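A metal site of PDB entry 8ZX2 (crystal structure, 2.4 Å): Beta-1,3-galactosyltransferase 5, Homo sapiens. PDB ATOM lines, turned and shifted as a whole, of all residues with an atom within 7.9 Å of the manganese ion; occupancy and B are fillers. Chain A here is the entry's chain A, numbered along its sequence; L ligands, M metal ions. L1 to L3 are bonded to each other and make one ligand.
O2 of LG3 L3 lies within hydrogen-bond range of OD1 of Asp 126, at 3.0 Å. O2 of LG3 L3 sits at hydrogen-bond distance from O of Gly 186.
The backbone carbonyl oxygen (O) of Pro 238 sits at hydrogen-bond distance from a ring nitrogen (ND1) of His 255 (3.1 Å). N of Phe 256 sits at hydrogen-bond distance from O of Asp 128 (3.2 Å). The backbone NH of Ile 257 is in hydrogen-bond range of the backbone carbonyl oxygen of Asp 128 (3.2 Å). N of Asp 126 is in hydrogen-bond range of O of Thr 187 (3.1 Å).
Within 4 Å of the manganese ion: Asp 126, Asp 128 and His 255. The nearest printed residue that does not touch the manganese ion is Thr 187 (5.2 Å).
The manganese ion is bound by NE2 of His 255 (2.3 Å), OD1 of Asp 128 (2.6 Å) and OD2 of Asp 126 (2.7 Å).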
ATOM      1  N   THR A  34      15.427  -7.262   8.285  1.00  0.00           N
ATOM      2  CA  THR A  34      16.299  -7.484   9.422  1.00  0.00           C
ATOM      3  C   THR A  34      17.382  -6.419   9.434  1.00  0.00           C
ATOM      4  O   THR A  34      17.999  -6.118   8.400  1.00  0.00           O
ATOM      5  CB  THR A  34      16.927  -8.877   9.394  1.00  0.00           C
ATOM      6  OG1 THR A  34      17.627  -9.057   8.164  1.00  0.00           O
ATOM      7  CG2 THR A  34      15.841  -9.927   9.467  1.00  0.00           C
ATOM      8  N   GLN A  39      21.480   0.385  13.210  1.00  0.00           N
ATOM      9  CA  GLN A  39      21.334   0.647  11.777  1.00  0.00           C
ATOM     10  C   GLN A  39      20.118   1.480  11.478  1.00  0.00           C
ATOM     11  O   GLN A  39      19.373   1.203  10.530  1.00  0.00           O
ATOM     12  CB  GLN A  39      21.306  -0.673  11.023  1.00  0.00           C
ATOM     13  CG  GLN A  39      22.600  -1.440  11.144  1.00  0.00           C
ATOM     14  CD  GLN A  39      22.632  -2.676  10.257  1.00  0.00           C
ATOM     15  OE1 GLN A  39      21.826  -3.580  10.412  1.00  0.00           O
ATOM     16  NE2 GLN A  39      23.591  -2.715   9.348  1.00  0.00           N
ATOM     17  N   TYR A  98      24.431 -11.087  15.675  1.00  0.00           N
ATOM     18  CA  TYR A  98      24.521 -11.869  14.448  1.00  0.00           C
ATOM     19  C   TYR A  98      24.145 -13.340  14.687  1.00  0.00           C
ATOM     20  O   TYR A  98      23.399 -13.930  13.896  1.00  0.00           O
ATOM     21  CB  TYR A  98      25.928 -11.764  13.861  1.00  0.00           C
ATOM     22  CG  TYR A  98      25.999 -12.270  12.436  1.00  0.00           C
ATOM     23  CD1 TYR A  98      25.515 -11.505  11.379  1.00  0.00           C
ATOM     24  CD2 TYR A  98      26.516 -13.538  12.152  1.00  0.00           C
ATOM     25  CE1 TYR A  98      25.552 -11.976  10.065  1.00  0.00           C
ATOM     26  CE2 TYR A  98      26.565 -14.016  10.835  1.00  0.00           C
ATOM     27  CZ  TYR A  98      26.083 -13.233   9.803  1.00  0.00           C
ATOM     28  OH  TYR A  98      26.132 -13.706   8.510  1.00  0.00           O
ATOM     29  N   ASP A 126      17.487  -8.379   4.052  1.00  0.00           N
ATOM     30  CA  ASP A 126      18.532  -7.635   4.739  1.00  0.00           C
ATOM     31  C   ASP A 126      18.347  -6.154   4.547  1.00  0.00           C
ATOM     32  O   ASP A 126      17.554  -5.682   3.723  1.00  0.00           O
ATOM     33  CB  ASP A 126      19.932  -7.904   4.208  1.00  0.00           C
ATOM     34  CG  ASP A 126      20.641  -9.085   4.843  1.00  0.00           C
ATOM     35  OD1 ASP A 126      20.006  -9.886   5.579  1.00  0.00           O
ATOM     36  OD2 ASP A 126      21.883  -9.140   4.624  1.00  0.00           O
ATOM     37  N   SER A 127      19.180  -5.408   5.262  1.00  0.00           N
ATOM     38  CA  SER A 127      19.098  -3.951   5.224  1.00  0.00           C
ATOM     39  C   SER A 127      19.929  -3.333   4.102  1.00  0.00           C
ATOM     40  O   SER A 127      19.578  -2.240   3.627  1.00  0.00           O
ATOM     41  CB  SER A 127      19.539  -3.391   6.583  1.00  0.00           C
ATOM     42  OG  SER A 127      20.820  -3.902   6.952  1.00  0.00           O
ATOM     43  N   ASP A 128      21.014  -3.959   3.650  1.00  0.00           N
ATOM     44  CA  ASP A 128      21.831  -3.319   2.616  1.00  0.00           C
ATOM     45  C   ASP A 128      21.439  -3.838   1.234  1.00  0.00           C
ATOM     46  O   ASP A 128      22.205  -4.529   0.540  1.00  0.00           O
ATOM     47  CB  ASP A 128      23.321  -3.504   2.885  1.00  0.00           C
ATOM     48  CG  ASP A 128      23.733  -4.974   2.972  1.00  0.00           C
ATOM     49  OD1 ASP A 128      22.900  -5.820   3.374  1.00  0.00           O
ATOM     50  OD2 ASP A 128      24.926  -5.255   2.697  1.00  0.00           O
ATOM     51  N   MET A 129      20.173  -3.566   0.885  1.00  0.00           N
ATOM     52  CA  MET A 129      19.520  -4.139  -0.276  1.00  0.00           C
ATOM     53  C   MET A 129      18.761  -3.075  -1.056  1.00  0.00           C
ATOM     54  O   MET A 129      18.198  -2.151  -0.475  1.00  0.00           O
ATOM     55  CB  MET A 129      18.504  -5.210   0.124  1.00  0.00           C
ATOM     56  CG  MET A 129      19.059  -6.443   0.841  1.00  0.00           C
ATOM     57  SD  MET A 129      19.936  -7.555  -0.267  1.00  0.00           S
ATOM     58  CE  MET A 129      18.641  -8.071  -1.338  1.00  0.00           C
ATOM     59  N   LYS A 167      33.114 -15.772   8.905  1.00  0.00           N
ATOM     60  CA  LYS A 167      31.897 -15.270   9.515  1.00  0.00           C
ATOM     61  C   LYS A 167      30.780 -16.310   9.513  1.00  0.00           C
ATOM     62  O   LYS A 167      29.942 -16.339  10.427  1.00  0.00           O
ATOM     63  CB  LYS A 167      31.440 -14.016   8.782  1.00  0.00           C
ATOM     64  CG  LYS A 167      29.956 -13.737   8.893  1.00  0.00           C
ATOM     65  CD  LYS A 167      29.540 -12.416   8.237  1.00  0.00           C
ATOM     66  CE  LYS A 167      29.444 -12.558   6.722  1.00  0.00           C
ATOM     67  NZ  LYS A 167      28.246 -11.800   6.216  1.00  0.00           N
ATOM     68  N   TRP A 168      30.752 -17.195   8.515  1.00  0.00           N
ATOM     69  CA  TRP A 168      29.734 -18.227   8.395  1.00  0.00           C
ATOM     70  C   TRP A 168      30.183 -19.595   8.893  1.00  0.00           C
ATOM     71  O   TRP A 168      29.544 -20.605   8.550  1.00  0.00           O
ATOM     72  CB  TRP A 168      29.268 -18.335   6.953  1.00  0.00           C
ATOM     73  CG  TRP A 168      28.700 -17.041   6.428  1.00  0.00           C
ATOM     74  CD1 TRP A 168      27.657 -16.332   6.957  1.00  0.00           C
ATOM     75  CD2 TRP A 168      29.131 -16.327   5.266  1.00  0.00           C
ATOM     76  NE1 TRP A 168      27.427 -15.211   6.197  1.00  0.00           N
ATOM     77  CE2 TRP A 168      28.320 -15.183   5.160  1.00  0.00           C
ATOM     78  CE3 TRP A 168      30.138 -16.539   4.324  1.00  0.00           C
ATOM     79  CZ2 TRP A 168      28.479 -14.250   4.125  1.00  0.00           C
ATOM     80  CZ3 TRP A 168      30.292 -15.612   3.295  1.00  0.00           C
ATOM     81  CH2 TRP A 168      29.460 -14.483   3.209  1.00  0.00           C
ATOM     82  N   GLY A 186      19.642 -15.521   2.406  1.00  0.00           N
ATOM     83  CA  GLY A 186      18.918 -14.680   3.367  1.00  0.00           C
ATOM     84  C   GLY A 186      19.038 -13.210   3.058  1.00  0.00           C
ATOM     85  O   GLY A 186      18.446 -12.431   3.782  1.00  0.00           O
ATOM     86  N   THR A 187      19.748 -12.849   1.984  1.00  0.00           N
ATOM     87  CA  THR A 187      19.793 -11.444   1.527  1.00  0.00           C
ATOM     88  C   THR A 187      18.392 -10.990   1.187  1.00  0.00           C
ATOM     89  O   THR A 187      18.092  -9.828   1.401  1.00  0.00           O
ATOM     90  CB  THR A 187      20.736 -11.335   0.330  1.00  0.00           C
ATOM     91  OG1 THR A 187      20.393 -12.339  -0.616  1.00  0.00           O
ATOM     92  CG2 THR A 187      22.192 -11.479   0.735  1.00  0.00           C
ATOM     93  N   PRO A 238      22.513 -11.781  -4.748  1.00  0.00           N
ATOM     94  CA  PRO A 238      23.302 -11.647  -3.522  1.00  0.00           C
ATOM     95  C   PRO A 238      24.698 -11.149  -3.777  1.00  0.00           C
ATOM     96  O   PRO A 238      25.304 -10.580  -2.855  1.00  0.00           O
ATOM     97  CB  PRO A 238      23.314 -13.083  -2.933  1.00  0.00           C
ATOM     98  CG  PRO A 238      22.149 -13.749  -3.577  1.00  0.00           C
ATOM     99  CD  PRO A 238      22.024 -13.153  -4.938  1.00  0.00           C
ATOM    100  N   HIS A 255      22.014  -6.923  -3.503  1.00  0.00           N
ATOM    101  CA  HIS A 255      22.728  -6.821  -2.244  1.00  0.00           C
ATOM    102  C   HIS A 255      23.938  -5.897  -2.383  1.00  0.00           C
ATOM    103  O   HIS A 255      24.274  -5.444  -3.484  1.00  0.00           O
ATOM    104  CB  HIS A 255      23.120  -8.235  -1.805  1.00  0.00           C
ATOM    105  CG  HIS A 255      23.716  -8.366  -0.448  1.00  0.00           C
ATOM    106  ND1 HIS A 255      24.813  -9.163  -0.193  1.00  0.00           N
ATOM    107  CD2 HIS A 255      23.321  -7.876   0.758  1.00  0.00           C
ATOM    108  CE1 HIS A 255      25.093  -9.139   1.097  1.00  0.00           C
ATOM    109  NE2 HIS A 255      24.199  -8.373   1.705  1.00  0.00           N
ATOM    110  N   PHE A 256      24.583  -5.601  -1.232  1.00  0.00           N
ATOM    111  CA  PHE A 256      25.779  -4.776  -1.125  1.00  0.00           C
ATOM    112  C   PHE A 256      25.490  -3.316  -1.460  1.00  0.00           C
ATOM    113  O   PHE A 256      26.256  -2.659  -2.159  1.00  0.00           O
ATOM    114  CB  PHE A 256      26.926  -5.305  -2.003  1.00  0.00           C
ATOM    115  CG  PHE A 256      27.476  -6.654  -1.575  1.00  0.00           C
ATOM    116  CD1 PHE A 256      27.901  -6.878  -0.284  1.00  0.00           C
ATOM    117  CD2 PHE A 256      27.550  -7.706  -2.479  1.00  0.00           C
ATOM    118  CE1 PHE A 256      28.402  -8.110   0.088  1.00  0.00           C
ATOM    119  CE2 PHE A 256      28.039  -8.944  -2.105  1.00  0.00           C
ATOM    120  CZ  PHE A 256      28.473  -9.140  -0.825  1.00  0.00           C
ATOM    121  N   ILE A 257      24.398  -2.782  -0.923  1.00  0.00           N
ATOM    122  CA  ILE A 257      23.927  -1.426  -1.206  1.00  0.00           C
ATOM    123  C   ILE A 257      23.814  -0.655   0.096  1.00  0.00           C
ATOM    124  O   ILE A 257      22.863  -0.867   0.864  1.00  0.00           O
ATOM    125  CB  ILE A 257      22.561  -1.439  -1.927  1.00  0.00           C
ATOM    126  CG1 ILE A 257      22.558  -2.434  -3.082  1.00  0.00           C
ATOM    127  CG2 ILE A 257      22.200  -0.038  -2.414  1.00  0.00           C
ATOM    128  CD1 ILE A 257      23.412  -2.000  -4.235  1.00  0.00           C
HETATM  129  C1  LIG L   1      28.845 -19.769  -2.042  1.00  0.00           C
HETATM  130  C2  LIG L   1      28.719 -18.452  -2.853  1.00  0.00           C
HETATM  131  C3  LIG L   1      29.299 -17.272  -2.039  1.00  0.00           C
HETATM  132  C4  LIG L   1      28.768 -17.247  -0.592  1.00  0.00           C
HETATM  133  C5  LIG L   1      28.960 -18.642   0.075  1.00  0.00           C
HETATM  134  C6  LIG L   1      28.388 -18.694   1.469  1.00  0.00           C
HETATM  135  O1  LIG L   1      28.152 -20.770  -2.751  1.00  0.00           O
HETATM  136  O2  LIG L   1      27.363 -18.147  -3.165  1.00  0.00           O
HETATM  137  O3  LIG L   1      29.076 -16.019  -2.680  1.00  0.00           O
HETATM  138  O4  LIG L   1      29.420 -16.232   0.162  1.00  0.00           O
HETATM  139  O5  LIG L   1      28.306 -19.667  -0.726  1.00  0.00           O
HETATM  140  O6  LIG L   1      27.281 -17.820   1.478  1.00  0.00           O
HETATM  141  C1  LG2 L   2      26.264 -18.396   2.315  1.00  0.00           C
HETATM  142  C2  LG2 L   2      25.200 -17.305   2.487  1.00  0.00           C
HETATM  143  C3  LG2 L   2      24.810 -17.228   3.932  1.00  0.00           C
HETATM  144  C4  LG2 L   2      24.613 -18.651   4.497  1.00  0.00           C
HETATM  145  C5  LG2 L   2      26.012 -19.288   4.571  1.00  0.00           C
HETATM  146  C6  LG2 L   2      26.072 -20.811   4.493  1.00  0.00           C
HETATM  147  O1  LG2 L   2      23.972 -17.646   1.782  1.00  0.00           O
HETATM  148  O2  LG2 L   2      23.622 -16.499   4.053  1.00  0.00           O
HETATM  149  O3  LG2 L   2      24.072 -18.548   5.795  1.00  0.00           O
HETATM  150  O4  LG2 L   2      26.850 -18.777   3.524  1.00  0.00           O
HETATM  151  O5  LG2 L   2      27.495 -21.167   4.592  1.00  0.00           O
HETATM  152  C1  LG3 L   3      23.683 -15.561   5.139  1.00  0.00           C
HETATM  153  C2  LG3 L   3      22.658 -14.474   4.760  1.00  0.00           C
HETATM  154  C3  LG3 L   3      22.375 -13.496   5.908  1.00  0.00           C
HETATM  155  C4  LG3 L   3      21.912 -14.320   7.135  1.00  0.00           C
HETATM  156  C5  LG3 L   3      23.022 -15.371   7.508  1.00  0.00           C
HETATM  157  C6  LG3 L   3      22.620 -16.429   8.581  1.00  0.00           C
HETATM  158  O1  LG3 L   3      23.032 -13.711   3.590  1.00  0.00           O
HETATM  159  O2  LG3 L   3      21.356 -12.547   5.548  1.00  0.00           O
HETATM  160  O3  LG3 L   3      20.689 -14.954   6.823  1.00  0.00           O
HETATM  161  O4  LG3 L   3      23.401 -16.187   6.365  1.00  0.00           O
HETATM  162  O5  LG3 L   3      22.185 -15.934   9.853  1.00  0.00           O
HETATM  163 MN    MN M   1      24.186  -7.982   3.969  1.00  0.00          MN
